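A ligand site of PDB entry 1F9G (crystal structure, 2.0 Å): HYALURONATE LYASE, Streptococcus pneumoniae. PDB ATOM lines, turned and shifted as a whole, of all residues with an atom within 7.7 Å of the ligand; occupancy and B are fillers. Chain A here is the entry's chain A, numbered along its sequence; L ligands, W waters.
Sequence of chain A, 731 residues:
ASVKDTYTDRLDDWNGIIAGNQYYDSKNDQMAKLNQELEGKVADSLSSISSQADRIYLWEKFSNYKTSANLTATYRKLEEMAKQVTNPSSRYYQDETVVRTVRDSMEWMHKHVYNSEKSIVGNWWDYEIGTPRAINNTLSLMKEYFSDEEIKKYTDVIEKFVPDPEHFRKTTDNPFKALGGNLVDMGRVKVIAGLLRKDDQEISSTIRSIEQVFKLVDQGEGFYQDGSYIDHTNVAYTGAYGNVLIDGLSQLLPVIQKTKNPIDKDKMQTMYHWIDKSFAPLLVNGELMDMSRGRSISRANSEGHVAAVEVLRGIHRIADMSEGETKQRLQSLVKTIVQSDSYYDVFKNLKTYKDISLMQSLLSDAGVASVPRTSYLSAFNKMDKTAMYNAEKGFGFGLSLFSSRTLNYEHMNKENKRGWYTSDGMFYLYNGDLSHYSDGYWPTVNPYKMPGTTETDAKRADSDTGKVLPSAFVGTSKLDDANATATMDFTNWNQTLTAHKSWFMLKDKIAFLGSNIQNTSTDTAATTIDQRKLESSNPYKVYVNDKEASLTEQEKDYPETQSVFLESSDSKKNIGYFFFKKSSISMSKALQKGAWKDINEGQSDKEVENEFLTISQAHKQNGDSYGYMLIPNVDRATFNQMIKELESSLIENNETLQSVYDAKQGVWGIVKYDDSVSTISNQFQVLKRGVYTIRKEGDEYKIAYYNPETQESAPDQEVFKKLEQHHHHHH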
ATOM      1  N   ALA A  69     -16.432 -24.865 -16.834  1.00  0.00           N
ATOM      2  CA  ALA A  69     -17.177 -23.849 -16.087  1.00  0.00           C
ATOM      3  C   ALA A  69     -18.292 -23.166 -16.905  1.00  0.00           C
ATOM      4  O   ALA A  69     -19.395 -22.973 -16.402  1.00  0.00           O
ATOM      5  CB  ALA A  69     -16.209 -22.801 -15.548  1.00  0.00           C
ATOM      6  N   THR A  72     -21.916 -24.921 -16.562  1.00  0.00           N
ATOM      7  CA  THR A  72     -22.824 -24.740 -15.437  1.00  0.00           C
ATOM      8  C   THR A  72     -23.097 -23.263 -15.137  1.00  0.00           C
ATOM      9  O   THR A  72     -24.056 -22.936 -14.452  1.00  0.00           O
ATOM     10  CB  THR A  72     -22.320 -25.437 -14.151  1.00  0.00           C
ATOM     11  OG1 THR A  72     -21.363 -24.604 -13.500  1.00  0.00           O
ATOM     12  CG2 THR A  72     -21.681 -26.774 -14.494  1.00  0.00           C
ATOM     13  N   ARG A  76     -26.840 -21.992 -14.780  1.00  0.00           N
ATOM     14  CA  ARG A  76     -27.083 -21.239 -13.553  1.00  0.00           C
ATOM     15  C   ARG A  76     -27.939 -20.018 -13.914  1.00  0.00           C
ATOM     16  O   ARG A  76     -28.773 -19.561 -13.122  1.00  0.00           O
ATOM     17  CB  ARG A  76     -25.747 -20.775 -12.953  1.00  0.00           C
ATOM     18  CG  ARG A  76     -25.552 -21.059 -11.479  1.00  0.00           C
ATOM     19  CD  ARG A  76     -25.150 -22.509 -11.212  1.00  0.00           C
ATOM     20  NE  ARG A  76     -23.739 -22.667 -10.829  1.00  0.00           N
ATOM     21  CZ  ARG A  76     -23.318 -23.030  -9.620  1.00  0.00           C
ATOM     22  NH1 ARG A  76     -22.016 -23.163  -9.375  1.00  0.00           N
ATOM     23  NH2 ARG A  76     -24.173 -23.256  -8.639  1.00  0.00           N
ATOM     24  N   ASN A 123     -13.397 -30.045 -16.332  1.00  0.00           N
ATOM     25  CA  ASN A 123     -13.616 -30.699 -15.036  1.00  0.00           C
ATOM     26  C   ASN A 123     -14.856 -31.596 -15.098  1.00  0.00           C
ATOM     27  O   ASN A 123     -15.853 -31.256 -15.738  1.00  0.00           O
ATOM     28  CB  ASN A 123     -13.775 -29.659 -13.923  1.00  0.00           C
ATOM     29  CG  ASN A 123     -13.224 -30.153 -12.581  1.00  0.00           C
ATOM     30  OD1 ASN A 123     -12.069 -30.555 -12.481  1.00  0.00           O
ATOM     31  ND2 ASN A 123     -14.069 -30.130 -11.555  1.00  0.00           N
ATOM     32  N   TRP A 124     -14.768 -32.742 -14.443  1.00  0.00           N
ATOM     33  CA  TRP A 124     -15.877 -33.689 -14.404  1.00  0.00           C
ATOM     34  C   TRP A 124     -17.010 -33.104 -13.548  1.00  0.00           C
ATOM     35  O   TRP A 124     -18.191 -33.372 -13.781  1.00  0.00           O
ATOM     36  CB  TRP A 124     -15.389 -34.997 -13.767  1.00  0.00           C
ATOM     37  CG  TRP A 124     -15.023 -34.790 -12.337  1.00  0.00           C
ATOM     38  CD1 TRP A 124     -13.850 -34.266 -11.855  1.00  0.00           C
ATOM     39  CD2 TRP A 124     -15.875 -34.966 -11.197  1.00  0.00           C
ATOM     40  NE1 TRP A 124     -13.930 -34.108 -10.486  1.00  0.00           N
ATOM     41  CE2 TRP A 124     -15.159 -34.528 -10.057  1.00  0.00           C
ATOM     42  CE3 TRP A 124     -17.178 -35.454 -11.027  1.00  0.00           C
ATOM     43  CZ2 TRP A 124     -15.711 -34.559  -8.772  1.00  0.00           C
ATOM     44  CZ3 TRP A 124     -17.717 -35.488  -9.745  1.00  0.00           C
ATOM     45  CH2 TRP A 124     -16.984 -35.038  -8.637  1.00  0.00           C
ATOM     46  N   TRP A 125     -16.624 -32.308 -12.551  1.00  0.00           N
ATOM     47  CA  TRP A 125     -17.543 -31.676 -11.614  1.00  0.00           C
ATOM     48  C   TRP A 125     -18.730 -31.001 -12.284  1.00  0.00           C
ATOM     49  O   TRP A 125     -19.863 -31.109 -11.807  1.00  0.00           O
ATOM     50  CB  TRP A 125     -16.789 -30.662 -10.752  1.00  0.00           C
ATOM     51  CG  TRP A 125     -17.542 -30.192  -9.560  1.00  0.00           C
ATOM     52  CD1 TRP A 125     -17.548 -30.764  -8.316  1.00  0.00           C
ATOM     53  CD2 TRP A 125     -18.425 -29.063  -9.480  1.00  0.00           C
ATOM     54  NE1 TRP A 125     -18.371 -30.065  -7.471  1.00  0.00           N
ATOM     55  CE2 TRP A 125     -18.922 -29.011  -8.158  1.00  0.00           C
ATOM     56  CE3 TRP A 125     -18.840 -28.088 -10.401  1.00  0.00           C
ATOM     57  CZ2 TRP A 125     -19.814 -28.020  -7.737  1.00  0.00           C
ATOM     58  CZ3 TRP A 125     -19.731 -27.104  -9.974  1.00  0.00           C
ATOM     59  CH2 TRP A 125     -20.205 -27.081  -8.652  1.00  0.00           C
ATOM     60  N   ASP A 126     -18.477 -30.313 -13.395  1.00  0.00           N
ATOM     61  CA  ASP A 126     -19.522 -29.604 -14.121  1.00  0.00           C
ATOM     62  C   ASP A 126     -20.459 -30.521 -14.897  1.00  0.00           C
ATOM     63  O   ASP A 126     -21.646 -30.218 -15.050  1.00  0.00           O
ATOM     64  CB  ASP A 126     -18.885 -28.611 -15.089  1.00  0.00           C
ATOM     65  CG  ASP A 126     -18.280 -27.428 -14.380  1.00  0.00           C
ATOM     66  OD1 ASP A 126     -19.020 -26.701 -13.677  1.00  0.00           O
ATOM     67  OD2 ASP A 126     -17.048 -27.207 -14.528  1.00  0.00           O
ATOM     68  N   ILE A 129     -22.016 -32.655 -11.437  1.00  0.00           N
ATOM     69  CA  ILE A 129     -22.620 -31.968 -10.303  1.00  0.00           C
ATOM     70  C   ILE A 129     -23.177 -30.581 -10.639  1.00  0.00           C
ATOM     71  O   ILE A 129     -24.401 -30.378 -10.638  1.00  0.00           O
ATOM     72  CB  ILE A 129     -21.624 -31.862  -9.133  1.00  0.00           C
ATOM     73  CG1 ILE A 129     -21.005 -33.238  -8.858  1.00  0.00           C
ATOM     74  CG2 ILE A 129     -22.325 -31.346  -7.884  1.00  0.00           C
ATOM     75  CD1 ILE A 129     -19.947 -33.244  -7.771  1.00  0.00           C
ATOM     76  N   GLY A 130     -22.296 -29.631 -10.932  1.00  0.00           N
ATOM     77  CA  GLY A 130     -22.731 -28.281 -11.251  1.00  0.00           C
ATOM     78  C   GLY A 130     -23.929 -28.219 -12.196  1.00  0.00           C
ATOM     79  O   GLY A 130     -25.037 -27.876 -11.784  1.00  0.00           O
ATOM     80  N   ARG A 133     -27.269 -30.127 -11.454  1.00  0.00           N
ATOM     81  CA  ARG A 133     -27.978 -29.503 -10.336  1.00  0.00           C
ATOM     82  C   ARG A 133     -28.776 -28.291 -10.820  1.00  0.00           C
ATOM     83  O   ARG A 133     -29.914 -28.096 -10.411  1.00  0.00           O
ATOM     84  CB  ARG A 133     -26.976 -29.062  -9.273  1.00  0.00           C
ATOM     85  CG  ARG A 133     -26.844 -30.018  -8.086  1.00  0.00           C
ATOM     86  CD  ARG A 133     -25.716 -29.594  -7.169  1.00  0.00           C
ATOM     87  NE  ARG A 133     -25.961 -28.288  -6.563  1.00  0.00           N
ATOM     88  CZ  ARG A 133     -25.013 -27.448  -6.183  1.00  0.00           C
ATOM     89  NH1 ARG A 133     -23.733 -27.746  -6.334  1.00  0.00           N
ATOM     90  NH2 ARG A 133     -25.339 -26.276  -5.648  1.00  0.00           N
ATOM     91  N   ASN A 182     -19.161 -34.444  -1.727  1.00  0.00           N
ATOM     92  CA  ASN A 182     -19.531 -34.933  -3.053  1.00  0.00           C
ATOM     93  C   ASN A 182     -20.683 -35.948  -3.010  1.00  0.00           C
ATOM     94  O   ASN A 182     -21.501 -36.008  -3.932  1.00  0.00           O
ATOM     95  CB  ASN A 182     -18.303 -35.560  -3.746  1.00  0.00           C
ATOM     96  CG  ASN A 182     -17.246 -34.537  -4.141  1.00  0.00           C
ATOM     97  OD1 ASN A 182     -16.046 -34.822  -4.109  1.00  0.00           O
ATOM     98  ND2 ASN A 182     -17.681 -33.333  -4.490  1.00  0.00           N
ATOM     99  N   ASP A 185     -23.770 -33.970  -2.742  1.00  0.00           N
ATOM    100  CA  ASP A 185     -24.087 -33.354  -4.015  1.00  0.00           C
ATOM    101  C   ASP A 185     -24.706 -34.398  -4.938  1.00  0.00           C
ATOM    102  O   ASP A 185     -25.457 -34.062  -5.855  1.00  0.00           O
ATOM    103  CB  ASP A 185     -22.829 -32.732  -4.626  1.00  0.00           C
ATOM    104  CG  ASP A 185     -22.795 -31.205  -4.482  1.00  0.00           C
ATOM    105  OD1 ASP A 185     -23.853 -30.616  -4.168  1.00  0.00           O
ATOM    106  OD2 ASP A 185     -21.720 -30.584  -4.669  1.00  0.00           O
ATOM    107  N   HIS A 232     -10.360 -35.308  -0.062  1.00  0.00           N
ATOM    108  CA  HIS A 232      -9.291 -35.342  -1.037  1.00  0.00           C
ATOM    109  C   HIS A 232      -8.155 -36.211  -0.483  1.00  0.00           C
ATOM    110  O   HIS A 232      -7.002 -35.796  -0.468  1.00  0.00           O
ATOM    111  CB  HIS A 232      -8.797 -33.939  -1.322  1.00  0.00           C
ATOM    112  CG  HIS A 232      -9.669 -33.188  -2.265  1.00  0.00           C
ATOM    113  ND1 HIS A 232      -9.284 -32.006  -2.859  1.00  0.00           N
ATOM    114  CD2 HIS A 232     -10.913 -33.458  -2.736  1.00  0.00           C
ATOM    115  CE1 HIS A 232     -10.252 -31.591  -3.665  1.00  0.00           C
ATOM    116  NE2 HIS A 232     -11.243 -32.455  -3.605  1.00  0.00           N
ATOM    117  N   TYR A 241     -15.364 -28.558   2.171  1.00  0.00           N
ATOM    118  CA  TYR A 241     -16.171 -29.711   1.776  1.00  0.00           C
ATOM    119  C   TYR A 241     -17.146 -30.093   2.888  1.00  0.00           C
ATOM    120  O   TYR A 241     -18.205 -30.672   2.627  1.00  0.00           O
ATOM    121  CB  TYR A 241     -15.255 -30.879   1.392  1.00  0.00           C
ATOM    122  CG  TYR A 241     -14.655 -30.685   0.012  1.00  0.00           C
ATOM    123  CD1 TYR A 241     -15.378 -31.050  -1.126  1.00  0.00           C
ATOM    124  CD2 TYR A 241     -13.418 -30.086  -0.159  1.00  0.00           C
ATOM    125  CE1 TYR A 241     -14.872 -30.817  -2.408  1.00  0.00           C
ATOM    126  CE2 TYR A 241     -12.891 -29.829  -1.433  1.00  0.00           C
ATOM    127  CZ  TYR A 241     -13.627 -30.198  -2.561  1.00  0.00           C
ATOM    128  OH  TYR A 241     -13.150 -29.936  -3.828  1.00  0.00           O
ATOM    129  N   VAL A 244     -20.199 -27.958   2.206  1.00  0.00           N
ATOM    130  CA  VAL A 244     -21.035 -28.540   1.153  1.00  0.00           C
ATOM    131  C   VAL A 244     -21.901 -29.647   1.711  1.00  0.00           C
ATOM    132  O   VAL A 244     -23.092 -29.758   1.393  1.00  0.00           O
ATOM    133  CB  VAL A 244     -20.185 -29.115  -0.005  1.00  0.00           C
ATOM    134  CG1 VAL A 244     -21.084 -29.801  -1.017  1.00  0.00           C
ATOM    135  CG2 VAL A 244     -19.400 -28.000  -0.664  1.00  0.00           C
ATOM    136  N   ARG A 295      -8.054 -24.854  -0.267  1.00  0.00           N
ATOM    137  CA  ARG A 295      -7.805 -23.939  -1.367  1.00  0.00           C
ATOM    138  C   ARG A 295      -8.809 -22.805  -1.528  1.00  0.00           C
ATOM    139  O   ARG A 295      -8.564 -21.868  -2.285  1.00  0.00           O
ATOM    140  CB  ARG A 295      -7.663 -24.721  -2.688  1.00  0.00           C
ATOM    141  CG  ARG A 295      -8.976 -25.101  -3.388  1.00  0.00           C
ATOM    142  CD  ARG A 295      -8.750 -26.146  -4.494  1.00  0.00           C
ATOM    143  NE  ARG A 295      -9.897 -26.251  -5.394  1.00  0.00           N
ATOM    144  CZ  ARG A 295     -10.712 -27.300  -5.464  1.00  0.00           C
ATOM    145  NH1 ARG A 295     -10.519 -28.360  -4.688  1.00  0.00           N
ATOM    146  NH2 ARG A 295     -11.738 -27.287  -6.295  1.00  0.00           N
ATOM    147  N   SER A 296      -9.920 -22.895  -0.811  1.00  0.00           N
ATOM    148  CA  SER A 296     -10.961 -21.873  -0.871  1.00  0.00           C
ATOM    149  C   SER A 296     -10.491 -20.531  -0.310  1.00  0.00           C
ATOM    150  O   SER A 296     -11.125 -19.505  -0.533  1.00  0.00           O
ATOM    151  CB  SER A 296     -12.189 -22.336  -0.108  1.00  0.00           C
ATOM    152  OG  SER A 296     -12.971 -23.177  -0.925  1.00  0.00           O
ATOM    153  N   ARG A 299     -10.166 -17.638  -2.795  1.00  0.00           N
ATOM    154  CA  ARG A 299     -11.334 -17.140  -3.514  1.00  0.00           C
ATOM    155  C   ARG A 299     -11.771 -15.820  -2.859  1.00  0.00           C
ATOM    156  O   ARG A 299     -12.071 -15.779  -1.665  1.00  0.00           O
ATOM    157  CB  ARG A 299     -12.467 -18.162  -3.450  1.00  0.00           C
ATOM    158  CG  ARG A 299     -12.156 -19.458  -4.160  1.00  0.00           C
ATOM    159  CD  ARG A 299     -13.179 -20.550  -3.847  1.00  0.00           C
ATOM    160  NE  ARG A 299     -12.743 -21.832  -4.381  1.00  0.00           N
ATOM    161  CZ  ARG A 299     -13.564 -22.846  -4.669  1.00  0.00           C
ATOM    162  NH1 ARG A 299     -14.870 -22.721  -4.475  1.00  0.00           N
ATOM    163  NH2 ARG A 299     -13.074 -23.977  -5.170  1.00  0.00           N
ATOM    164  N   MET A 412      -4.826 -26.843  -6.238  1.00  0.00           N
ATOM    165  CA  MET A 412      -5.509 -27.609  -7.264  1.00  0.00           C
ATOM    166  C   MET A 412      -6.443 -26.742  -8.065  1.00  0.00           C
ATOM    167  O   MET A 412      -6.937 -25.742  -7.564  1.00  0.00           O
ATOM    168  CB  MET A 412      -6.289 -28.730  -6.611  1.00  0.00           C
ATOM    169  CG  MET A 412      -6.956 -29.674  -7.575  1.00  0.00           C
ATOM    170  SD  MET A 412      -7.939 -30.892  -6.688  1.00  0.00           S
ATOM    171  CE  MET A 412      -6.619 -31.782  -5.799  1.00  0.00           C
ATOM    172  N   ASN A 413      -6.677 -27.123  -9.318  1.00  0.00           N
ATOM    173  CA  ASN A 413      -7.562 -26.381 -10.213  1.00  0.00           C
ATOM    174  C   ASN A 413      -7.056 -24.951 -10.404  1.00  0.00           C
ATOM    175  O   ASN A 413      -7.829 -24.050 -10.702  1.00  0.00           O
ATOM    176  CB  ASN A 413      -8.990 -26.345  -9.670  1.00  0.00           C
ATOM    177  CG  ASN A 413      -9.787 -27.561 -10.056  1.00  0.00           C
ATOM    178  OD1 ASN A 413      -9.301 -28.443 -10.762  1.00  0.00           O
ATOM    179  ND2 ASN A 413     -11.033 -27.622  -9.599  1.00  0.00           N
ATOM    180  N   GLU A 415      -5.945 -23.050  -8.080  1.00  0.00           N
ATOM    181  CA  GLU A 415      -6.239 -22.251  -6.890  1.00  0.00           C
ATOM    182  C   GLU A 415      -5.224 -22.460  -5.775  1.00  0.00           C
ATOM    183  O   GLU A 415      -4.663 -23.548  -5.624  1.00  0.00           O
ATOM    184  CB  GLU A 415      -7.632 -22.580  -6.354  1.00  0.00           C
ATOM    185  CG  GLU A 415      -8.647 -22.904  -7.415  1.00  0.00           C
ATOM    186  CD  GLU A 415     -10.055 -22.935  -6.853  1.00  0.00           C
ATOM    187  OE1 GLU A 415     -10.640 -24.037  -6.747  1.00  0.00           O
ATOM    188  OE2 GLU A 415     -10.579 -21.851  -6.523  1.00  0.00           O
HETATM  189  C1  LIG L   1     -15.482 -27.591  -6.506  1.00  0.00           C
HETATM  190  C2  LIG L   1     -14.754 -27.468  -7.847  1.00  0.00           C
HETATM  191  C3  LIG L   1     -14.797 -26.200  -8.287  1.00  0.00           C
HETATM  192  C4  LIG L   1     -15.579 -25.397  -7.258  1.00  0.00           C
HETATM  193  C5  LIG L   1     -16.663 -24.467  -7.866  1.00  0.00           C
HETATM  194  C6  LIG L   1     -17.774 -23.750  -7.063  1.00  0.00           C
HETATM  195  O1  LIG L   1     -15.646 -28.568  -5.775  1.00  0.00           O
HETATM  196  O2  LIG L   1     -14.117 -28.467  -8.531  1.00  0.00           O
HETATM  197  O3  LIG L   1     -13.952 -25.554  -8.943  1.00  0.00           O
HETATM  198  O4  LIG L   1     -15.967 -26.335  -6.190  1.00  0.00           O
HETATM  199  O5  LIG L   1     -16.104 -23.557  -8.842  1.00  0.00           O
HETATM  200  O6  LIG L   1     -18.960 -23.886  -7.977  1.00  0.00           O
HETATM  201  O   HOH W   1     -14.900 -26.412  -2.956  1.00  0.00           O
HETATM  202  O   HOH W   2     -12.289 -30.778  -7.420  1.00  0.00           O
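An oxygen (O2) of the ligand is in hydrogen-bond range of the side-chain amide nitrogen (ND2) of Asn 413, 3.4 Å away. An oxygen (O2) of the ligand sits close to the guanidinium group of Arg 295 (3.5 Å). NH1 of Arg 76 is in hydrogen-bond range of O6 of the ligand, 3.4 Å away. An oxygen (O1) of the ligand sits at hydrogen-bond distance from the side-chain hydroxyl (OH) of Tyr 241 (3.4 Å). An oxygen (O2) of the ligand lies within hydrogen-bond range of the side-chain amide nitrogen (ND2) of Asn 123 (3.5 Å).
ND2 of Asn 413 lies close to NH2 of Arg 295 (3.4 Å). NH1 of Arg 295 lies within hydrogen-bond range of OH of Tyr 241 (3.2 Å). The guanidinium group (NE) of Arg 295 lies within salt-bridge range of the side-chain carboxylate (OE1) of Glu 415 (2.7 Å). The side-chain hydroxyl (OH) of Tyr 241 is in hydrogen-bond range of a ring nitrogen (NE2) of His 232 (3.2 Å). The backbone carbonyl oxygen of Trp 125 is in hydrogen-bond range of the backbone NH of Gly 130 (3.0 Å). OE1 of Glu 415 lies within salt-bridge range of NH2 of Arg 299 (2.9 Å).
Trp 125 touches the ligand (CH2 to O6, 3.5 Å). Arg 299 touches the ligand (NH2 to C4, 3.6 Å). Hydrophobic or aromatic side chains that line the ligand: Trp 125. Seven residues have an atom within 4 Å of the ligand: Arg 76, Asn 123, Trp 125, Tyr 241, Arg 295, Arg 299 and Asn 413. The nearest printed residue that does not touch the ligand is Glu 415 (4.3 Å).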
